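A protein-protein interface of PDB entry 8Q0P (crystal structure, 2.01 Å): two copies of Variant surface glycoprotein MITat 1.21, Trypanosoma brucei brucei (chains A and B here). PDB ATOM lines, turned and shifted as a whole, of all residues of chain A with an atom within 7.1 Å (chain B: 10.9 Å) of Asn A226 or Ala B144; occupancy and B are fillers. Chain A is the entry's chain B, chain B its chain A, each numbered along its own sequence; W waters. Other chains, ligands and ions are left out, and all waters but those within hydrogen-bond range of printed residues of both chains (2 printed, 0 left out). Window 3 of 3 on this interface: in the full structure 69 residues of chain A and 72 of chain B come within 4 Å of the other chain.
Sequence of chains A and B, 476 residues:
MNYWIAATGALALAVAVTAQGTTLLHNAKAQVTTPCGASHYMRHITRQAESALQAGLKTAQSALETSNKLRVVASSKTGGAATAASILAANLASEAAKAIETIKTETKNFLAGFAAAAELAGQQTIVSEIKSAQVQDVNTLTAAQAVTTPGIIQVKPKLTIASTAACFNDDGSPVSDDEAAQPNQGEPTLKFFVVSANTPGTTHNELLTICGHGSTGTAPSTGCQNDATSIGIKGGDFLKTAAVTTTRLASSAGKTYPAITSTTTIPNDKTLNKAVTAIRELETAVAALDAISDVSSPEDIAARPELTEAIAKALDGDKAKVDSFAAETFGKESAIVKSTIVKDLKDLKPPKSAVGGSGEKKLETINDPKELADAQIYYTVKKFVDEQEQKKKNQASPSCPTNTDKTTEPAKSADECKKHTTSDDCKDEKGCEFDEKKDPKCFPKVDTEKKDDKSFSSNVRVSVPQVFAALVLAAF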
ATOM      1  N   HIS A 204       5.462 -28.764  21.055  1.00  0.00           N
ATOM      2  CA  HIS A 204       6.755 -28.848  20.392  1.00  0.00           C
ATOM      3  C   HIS A 204       7.302 -30.269  20.448  1.00  0.00           C
ATOM      4  O   HIS A 204       7.097 -31.003  21.419  1.00  0.00           O
ATOM      5  CB  HIS A 204       7.756 -27.863  21.001  1.00  0.00           C
ATOM      6  CG  HIS A 204       7.976 -28.031  22.473  1.00  0.00           C
ATOM      7  ND1 HIS A 204       7.221 -27.371  23.418  1.00  0.00           N
ATOM      8  CD2 HIS A 204       8.879 -28.770  23.162  1.00  0.00           C
ATOM      9  CE1 HIS A 204       7.647 -27.698  24.627  1.00  0.00           C
ATOM     10  NE2 HIS A 204       8.652 -28.547  24.498  1.00  0.00           N
ATOM     11  N   GLY A 212      10.635 -25.308  16.540  1.00  0.00           N
ATOM     12  CA  GLY A 212      11.462 -24.228  17.049  1.00  0.00           C
ATOM     13  C   GLY A 212      12.781 -24.754  17.590  1.00  0.00           C
ATOM     14  O   GLY A 212      12.874 -25.888  18.050  1.00  0.00           O
ATOM     15  N   HIS A 213      13.820 -23.928  17.499  1.00  0.00           N
ATOM     16  CA  HIS A 213      15.074 -24.247  18.169  1.00  0.00           C
ATOM     17  C   HIS A 213      15.879 -22.972  18.370  1.00  0.00           C
ATOM     18  O   HIS A 213      15.812 -22.041  17.561  1.00  0.00           O
ATOM     19  CB  HIS A 213      15.903 -25.281  17.389  1.00  0.00           C
ATOM     20  CG  HIS A 213      16.849 -26.062  18.249  1.00  0.00           C
ATOM     21  ND1 HIS A 213      18.106 -25.604  18.576  1.00  0.00           N
ATOM     22  CD2 HIS A 213      16.715 -27.265  18.863  1.00  0.00           C
ATOM     23  CE1 HIS A 213      18.710 -26.489  19.351  1.00  0.00           C
ATOM     24  NE2 HIS A 213      17.889 -27.509  19.535  1.00  0.00           N
ATOM     25  N   GLY A 214      16.650 -22.948  19.458  1.00  0.00           N
ATOM     26  CA  GLY A 214      17.534 -21.828  19.714  1.00  0.00           C
ATOM     27  C   GLY A 214      18.694 -21.724  18.743  1.00  0.00           C
ATOM     28  O   GLY A 214      19.212 -20.625  18.531  1.00  0.00           O
ATOM     29  N   CYS A 224      12.804 -30.509  19.108  1.00  0.00           N
ATOM     30  CA  CYS A 224      12.334 -29.139  19.000  1.00  0.00           C
ATOM     31  C   CYS A 224      12.126 -28.541  20.386  1.00  0.00           C
ATOM     32  O   CYS A 224      11.885 -29.253  21.364  1.00  0.00           O
ATOM     33  CB  CYS A 224      11.040 -29.095  18.196  1.00  0.00           C
ATOM     34  SG  CYS A 224      11.196 -29.930  16.584  1.00  0.00           S
ATOM     35  N   GLN A 225      12.238 -27.217  20.468  1.00  0.00           N
ATOM     36  CA  GLN A 225      12.154 -26.513  21.738  1.00  0.00           C
ATOM     37  C   GLN A 225      11.124 -25.400  21.651  1.00  0.00           C
ATOM     38  O   GLN A 225      10.750 -24.951  20.569  1.00  0.00           O
ATOM     39  CB  GLN A 225      13.502 -25.911  22.155  1.00  0.00           C
ATOM     40  CG  GLN A 225      14.674 -26.806  21.896  1.00  0.00           C
ATOM     41  CD  GLN A 225      15.989 -26.104  22.125  1.00  0.00           C
ATOM     42  OE1 GLN A 225      16.201 -24.987  21.648  1.00  0.00           O
ATOM     43  NE2 GLN A 225      16.893 -26.761  22.852  1.00  0.00           N
ATOM     44  N   ASN A 226      10.684 -24.950  22.826  1.00  0.00           N
ATOM     45  CA  ASN A 226       9.892 -23.730  22.962  1.00  0.00           C
ATOM     46  C   ASN A 226      10.832 -22.543  22.783  1.00  0.00           C
ATOM     47  O   ASN A 226      11.216 -21.861  23.732  1.00  0.00           O
ATOM     48  CB  ASN A 226       9.195 -23.689  24.316  1.00  0.00           C
ATOM     49  CG  ASN A 226       8.335 -22.451  24.495  1.00  0.00           C
ATOM     50  OD1 ASN A 226       8.113 -21.684  23.555  1.00  0.00           O
ATOM     51  ND2 ASN A 226       7.846 -22.249  25.712  1.00  0.00           N
ATOM     52  N   ASP A 227      11.200 -22.288  21.531  1.00  0.00           N
ATOM     53  CA  ASP A 227      12.164 -21.236  21.206  1.00  0.00           C
ATOM     54  C   ASP A 227      12.061 -20.950  19.714  1.00  0.00           C
ATOM     55  O   ASP A 227      12.306 -21.847  18.900  1.00  0.00           O
ATOM     56  CB  ASP A 227      13.583 -21.682  21.562  1.00  0.00           C
ATOM     57  CG  ASP A 227      14.627 -20.599  21.326  1.00  0.00           C
ATOM     58  OD1 ASP A 227      14.507 -19.821  20.353  1.00  0.00           O
ATOM     59  OD2 ASP A 227      15.610 -20.562  22.102  1.00  0.00           O
ATOM     60  N   ALA A 228      11.751 -19.707  19.344  1.00  0.00           N
ATOM     61  CA  ALA A 228      11.483 -19.379  17.950  1.00  0.00           C
ATOM     62  C   ALA A 228      12.634 -18.635  17.277  1.00  0.00           C
ATOM     63  O   ALA A 228      12.419 -17.986  16.250  1.00  0.00           O
ATOM     64  CB  ALA A 228      10.189 -18.571  17.836  1.00  0.00           C
ATOM     65  N   THR A 229      13.850 -18.728  17.820  1.00  0.00           N
ATOM     66  CA  THR A 229      14.996 -18.090  17.176  1.00  0.00           C
ATOM     67  C   THR A 229      15.190 -18.619  15.758  1.00  0.00           C
ATOM     68  O   THR A 229      15.336 -17.842  14.806  1.00  0.00           O
ATOM     69  CB  THR A 229      16.257 -18.307  18.012  1.00  0.00           C
ATOM     70  OG1 THR A 229      16.014 -17.891  19.362  1.00  0.00           O
ATOM     71  CG2 THR A 229      17.432 -17.499  17.444  1.00  0.00           C
ATOM     72  N   THR B 140      -1.411 -17.112  10.672  1.00  0.00           N
ATOM     73  CA  THR B 140      -0.155 -16.784  11.325  1.00  0.00           C
ATOM     74  C   THR B 140      -0.366 -16.571  12.826  1.00  0.00           C
ATOM     75  O   THR B 140      -1.454 -16.203  13.284  1.00  0.00           O
ATOM     76  CB  THR B 140       0.467 -15.540  10.697  1.00  0.00           C
ATOM     77  OG1 THR B 140      -0.310 -14.392  11.057  1.00  0.00           O
ATOM     78  CG2 THR B 140       0.511 -15.672   9.166  1.00  0.00           C
ATOM     79  N   LEU B 141       0.685 -16.835  13.598  1.00  0.00           N
ATOM     80  CA  LEU B 141       0.685 -16.546  15.025  1.00  0.00           C
ATOM     81  C   LEU B 141       2.037 -15.964  15.411  1.00  0.00           C
ATOM     82  O   LEU B 141       3.070 -16.386  14.888  1.00  0.00           O
ATOM     83  CB  LEU B 141       0.371 -17.809  15.857  1.00  0.00           C
ATOM     84  CG  LEU B 141       0.224 -17.658  17.387  1.00  0.00           C
ATOM     85  CD1 LEU B 141      -0.831 -16.624  17.757  1.00  0.00           C
ATOM     86  CD2 LEU B 141      -0.085 -19.018  18.060  1.00  0.00           C
ATOM     87  N   THR B 142       2.018 -14.968  16.300  1.00  0.00           N
ATOM     88  CA  THR B 142       3.234 -14.418  16.897  1.00  0.00           C
ATOM     89  C   THR B 142       4.267 -15.513  17.137  1.00  0.00           C
ATOM     90  O   THR B 142       3.960 -16.546  17.736  1.00  0.00           O
ATOM     91  CB  THR B 142       2.876 -13.723  18.210  1.00  0.00           C
ATOM     92  OG1 THR B 142       1.939 -12.671  17.941  1.00  0.00           O
ATOM     93  CG2 THR B 142       4.119 -13.151  18.884  1.00  0.00           C
ATOM     94  N   ALA B 143       5.493 -15.288  16.649  1.00  0.00           N
ATOM     95  CA  ALA B 143       6.409 -16.413  16.434  1.00  0.00           C
ATOM     96  C   ALA B 143       6.691 -17.177  17.724  1.00  0.00           C
ATOM     97  O   ALA B 143       6.761 -18.412  17.716  1.00  0.00           O
ATOM     98  CB  ALA B 143       7.712 -15.931  15.802  1.00  0.00           C
ATOM     99  N   ALA B 144       6.842 -16.460  18.843  1.00  0.00           N
ATOM    100  CA  ALA B 144       7.160 -17.104  20.116  1.00  0.00           C
ATOM    101  C   ALA B 144       6.075 -18.080  20.552  1.00  0.00           C
ATOM    102  O   ALA B 144       6.382 -19.100  21.181  1.00  0.00           O
ATOM    103  CB  ALA B 144       7.382 -16.048  21.199  1.00  0.00           C
ATOM    104  N   GLN B 145       4.809 -17.795  20.229  1.00  0.00           N
ATOM    105  CA  GLN B 145       3.702 -18.696  20.537  1.00  0.00           C
ATOM    106  C   GLN B 145       3.460 -19.749  19.461  1.00  0.00           C
ATOM    107  O   GLN B 145       2.724 -20.713  19.712  1.00  0.00           O
ATOM    108  CB  GLN B 145       2.415 -17.899  20.744  1.00  0.00           C
ATOM    109  CG  GLN B 145       2.539 -16.778  21.775  1.00  0.00           C
ATOM    110  CD  GLN B 145       1.312 -15.892  21.800  1.00  0.00           C
ATOM    111  OE1 GLN B 145       0.182 -16.375  21.704  1.00  0.00           O
ATOM    112  NE2 GLN B 145       1.527 -14.587  21.923  1.00  0.00           N
ATOM    113  N   ALA B 146       4.044 -19.583  18.274  1.00  0.00           N
ATOM    114  CA  ALA B 146       3.827 -20.501  17.162  1.00  0.00           C
ATOM    115  C   ALA B 146       4.576 -21.820  17.305  1.00  0.00           C
ATOM    116  O   ALA B 146       4.314 -22.743  16.532  1.00  0.00           O
ATOM    117  CB  ALA B 146       4.244 -19.829  15.853  1.00  0.00           C
ATOM    118  N   VAL B 147       5.493 -21.940  18.260  1.00  0.00           N
ATOM    119  CA  VAL B 147       6.359 -23.109  18.354  1.00  0.00           C
ATOM    120  C   VAL B 147       6.032 -23.977  19.568  1.00  0.00           C
ATOM    121  O   VAL B 147       6.795 -24.890  19.887  1.00  0.00           O
ATOM    122  CB  VAL B 147       7.841 -22.698  18.374  1.00  0.00           C
ATOM    123  CG1 VAL B 147       8.239 -22.028  17.055  1.00  0.00           C
ATOM    124  CG2 VAL B 147       8.111 -21.770  19.555  1.00  0.00           C
ATOM    125  N   THR B 148       4.936 -23.710  20.276  1.00  0.00           N
ATOM    126  CA  THR B 148       4.623 -24.554  21.422  1.00  0.00           C
ATOM    127  C   THR B 148       3.132 -24.488  21.725  1.00  0.00           C
ATOM    128  O   THR B 148       2.395 -23.667  21.172  1.00  0.00           O
ATOM    129  CB  THR B 148       5.462 -24.156  22.643  1.00  0.00           C
ATOM    130  OG1 THR B 148       5.399 -25.200  23.621  1.00  0.00           O
ATOM    131  CG2 THR B 148       4.962 -22.840  23.244  1.00  0.00           C
ATOM    132  N   THR B 149       2.693 -25.393  22.604  1.00  0.00           N
ATOM    133  CA  THR B 149       1.312 -25.385  23.054  1.00  0.00           C
ATOM    134  C   THR B 149       1.022 -24.063  23.769  1.00  0.00           C
ATOM    135  O   THR B 149       1.916 -23.473  24.383  1.00  0.00           O
ATOM    136  CB  THR B 149       1.050 -26.574  23.983  1.00  0.00           C
ATOM    137  OG1 THR B 149      -0.355 -26.695  24.236  1.00  0.00           O
ATOM    138  CG2 THR B 149       1.791 -26.421  25.302  1.00  0.00           C
ATOM    139  N   PRO B 150      -0.213 -23.543  23.675  1.00  0.00           N
ATOM    140  CA  PRO B 150      -1.372 -24.078  22.954  1.00  0.00           C
ATOM    141  C   PRO B 150      -1.479 -23.634  21.489  1.00  0.00           C
ATOM    142  O   PRO B 150      -2.374 -24.105  20.790  1.00  0.00           O
ATOM    143  CB  PRO B 150      -2.546 -23.533  23.767  1.00  0.00           C
ATOM    144  CG  PRO B 150      -2.059 -22.191  24.249  1.00  0.00           C
ATOM    145  CD  PRO B 150      -0.552 -22.307  24.407  1.00  0.00           C
ATOM    146  N   GLY B 151      -0.589 -22.761  21.017  1.00  0.00           N
ATOM    147  CA  GLY B 151      -0.760 -22.222  19.678  1.00  0.00           C
ATOM    148  C   GLY B 151       0.069 -22.826  18.554  1.00  0.00           C
ATOM    149  O   GLY B 151       0.114 -22.253  17.463  1.00  0.00           O
ATOM    150  N   ILE B 152       0.718 -23.972  18.786  1.00  0.00           N
ATOM    151  CA  ILE B 152       1.719 -24.464  17.844  1.00  0.00           C
ATOM    152  C   ILE B 152       1.101 -24.587  16.458  1.00  0.00           C
ATOM    153  O   ILE B 152      -0.011 -25.105  16.290  1.00  0.00           O
ATOM    154  CB  ILE B 152       2.316 -25.797  18.327  1.00  0.00           C
ATOM    155  CG1 ILE B 152       3.522 -26.187  17.467  1.00  0.00           C
ATOM    156  CG2 ILE B 152       1.284 -26.923  18.283  1.00  0.00           C
ATOM    157  CD1 ILE B 152       4.545 -27.027  18.195  1.00  0.00           C
ATOM    158  N   ILE B 153       1.799 -24.041  15.466  1.00  0.00           N
ATOM    159  CA  ILE B 153       1.365 -24.143  14.079  1.00  0.00           C
ATOM    160  C   ILE B 153       1.558 -25.574  13.597  1.00  0.00           C
ATOM    161  O   ILE B 153       2.654 -26.136  13.704  1.00  0.00           O
ATOM    162  CB  ILE B 153       2.156 -23.155  13.215  1.00  0.00           C
ATOM    163  CG1 ILE B 153       1.955 -21.716  13.726  1.00  0.00           C
ATOM    164  CG2 ILE B 153       1.794 -23.321  11.770  1.00  0.00           C
ATOM    165  CD1 ILE B 153       0.539 -21.168  13.545  1.00  0.00           C
ATOM    166  N   HIS B 213       3.902 -13.043   8.324  1.00  0.00           N
ATOM    167  CA  HIS B 213       3.120 -11.818   8.231  1.00  0.00           C
ATOM    168  C   HIS B 213       3.464 -10.897   9.390  1.00  0.00           C
ATOM    169  O   HIS B 213       3.779 -11.352  10.494  1.00  0.00           O
ATOM    170  CB  HIS B 213       1.612 -12.096   8.214  1.00  0.00           C
ATOM    171  CG  HIS B 213       0.817 -11.005   7.573  1.00  0.00           C
ATOM    172  ND1 HIS B 213       0.416  -9.872   8.253  1.00  0.00           N
ATOM    173  CD2 HIS B 213       0.382 -10.854   6.298  1.00  0.00           C
ATOM    174  CE1 HIS B 213      -0.243  -9.076   7.428  1.00  0.00           C
ATOM    175  NE2 HIS B 213      -0.276  -9.648   6.234  1.00  0.00           N
ATOM    176  N   THR B 216      -0.153 -10.859  13.466  1.00  0.00           N
ATOM    177  CA  THR B 216      -0.609 -12.158  13.939  1.00  0.00           C
ATOM    178  C   THR B 216      -2.098 -12.332  13.636  1.00  0.00           C
ATOM    179  O   THR B 216      -2.863 -11.365  13.581  1.00  0.00           O
ATOM    180  CB  THR B 216      -0.320 -12.311  15.442  1.00  0.00           C
ATOM    181  OG1 THR B 216      -0.650 -13.638  15.870  1.00  0.00           O
ATOM    182  CG2 THR B 216      -1.108 -11.306  16.270  1.00  0.00           C
ATOM    183  N   ALA B 228       8.740 -12.142   9.620  1.00  0.00           N
ATOM    184  CA  ALA B 228       8.648 -13.271  10.537  1.00  0.00           C
ATOM    185  C   ALA B 228       8.090 -12.885  11.906  1.00  0.00           C
ATOM    186  O   ALA B 228       8.240 -13.653  12.866  1.00  0.00           O
ATOM    187  CB  ALA B 228      10.013 -13.949  10.686  1.00  0.00           C
ATOM    188  N   THR B 229       7.429 -11.726  12.014  1.00  0.00           N
ATOM    189  CA  THR B 229       6.780 -11.356  13.271  1.00  0.00           C
ATOM    190  C   THR B 229       5.769 -12.420  13.687  1.00  0.00           C
ATOM    191  O   THR B 229       5.733 -12.851  14.849  1.00  0.00           O
ATOM    192  CB  THR B 229       6.106  -9.994  13.122  1.00  0.00           C
ATOM    193  OG1 THR B 229       7.074  -9.050  12.648  1.00  0.00           O
ATOM    194  CG2 THR B 229       5.533  -9.513  14.466  1.00  0.00           C
ATOM    195  N   SER B 230       4.959 -12.877  12.743  1.00  0.00           N
ATOM    196  CA  SER B 230       4.073 -14.006  12.968  1.00  0.00           C
ATOM    197  C   SER B 230       4.272 -15.002  11.836  1.00  0.00           C
ATOM    198  O   SER B 230       4.685 -14.637  10.734  1.00  0.00           O
ATOM    199  CB  SER B 230       2.603 -13.558  13.064  1.00  0.00           C
ATOM    200  OG  SER B 230       2.139 -13.023  11.836  1.00  0.00           O
ATOM    201  N   ILE B 231       4.008 -16.271  12.117  1.00  0.00           N
ATOM    202  CA  ILE B 231       4.213 -17.321  11.131  1.00  0.00           C
ATOM    203  C   ILE B 231       3.013 -18.249  11.126  1.00  0.00           C
ATOM    204  O   ILE B 231       2.432 -18.547  12.177  1.00  0.00           O
ATOM    205  CB  ILE B 231       5.513 -18.119  11.375  1.00  0.00           C
ATOM    206  CG1 ILE B 231       5.472 -18.824  12.727  1.00  0.00           C
ATOM    207  CG2 ILE B 231       6.751 -17.220  11.243  1.00  0.00           C
ATOM    208  CD1 ILE B 231       6.846 -19.237  13.232  1.00  0.00           C
ATOM    209  N   GLY B 232       2.635 -18.687   9.930  1.00  0.00           N
ATOM    210  CA  GLY B 232       1.609 -19.686   9.747  1.00  0.00           C
ATOM    211  C   GLY B 232       2.054 -20.666   8.682  1.00  0.00           C
ATOM    212  O   GLY B 232       3.256 -20.852   8.459  1.00  0.00           O
HETATM  213  O   HOH W   1       8.710 -26.463  18.318  1.00  0.00           O
HETATM  214  O   HOH W   2       8.765 -19.491  22.357  1.00  0.00           O
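Water W2 lies within hydrogen-bond range of OD1 of Asn A226 (2.6 Å) and O of Ala B144 (2.7 Å). Water W1 lies within hydrogen-bond range of the backbone NH of Gly A212 (2.9 Å), the backbone carbonyl oxygen of Val B147 (2.9 Å) and the backbone carbonyl oxygen of Gln A225 (3.4 Å).
Ala B144 touches one residue of chain A. Gly A212 touches one residue of chain B. Of chain B, only Val B147 (3.7 Å) comes within 4 Å of Asp A227. Ala A228 touches one residue of chain B. Of the printed residues of chain A, Thr B148 touches His A204 and Asn A226. Printed residues of chain B within 4 Å of His A204: Val B147, Thr B148 and Ile B152. Printed residues of chain A within 4 Å of Ile B152: His A204 (3.5 Å). Gly A214 touches none of the printed residues of chain B. The nearest printed residue of chain B that does not touch Asn A226 is Val B147 (4.001 Å).
Among the printed residues, pairs that only touch across the chains: His A204 with Val B147 (3.3 Å), Asn A226 with Thr B148 (3.4 Å), Ala A228 with Ala B143 (3.4 Å), His A204 with Ile B152 (3.5 Å), Asp A227 with Val B147 (3.7 Å), Gly A212 with Val B147 (3.9 Å) and Asn A226 with Ala B144 (3.9 Å).
A ring nitrogen (ND1) of His A204 lies within hydrogen-bond range of the side-chain hydroxyl of Thr B148 (2.8 Å).
The side-chain hydroxyl (OG1) of Thr A229 is in hydrogen-bond range of the side-chain carboxylate (OD1) of Asp A227 (2.6 Å). The backbone NH (N) of Gln A225 sits at hydrogen-bond distance from the backbone carbonyl oxygen (O) of Gly A212 (2.8 Å). The backbone NH (N) of Ala B143 lies within hydrogen-bond range of the backbone carbonyl oxygen (O) of Thr B229 (3.0 Å). The backbone carbonyl oxygen (O) of Asp A227 is in hydrogen-bond range of the backbone NH (N) of His A213, at 2.9 Å.
Positions printed for both chains: 213, 228 and 229.
Of the 10 printed residues of chain A, 5 touch a printed residue of chain B. Hydrophobic or aromatic side chains of chain A that line the printed part of chain B: His A204 and Ala A228.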
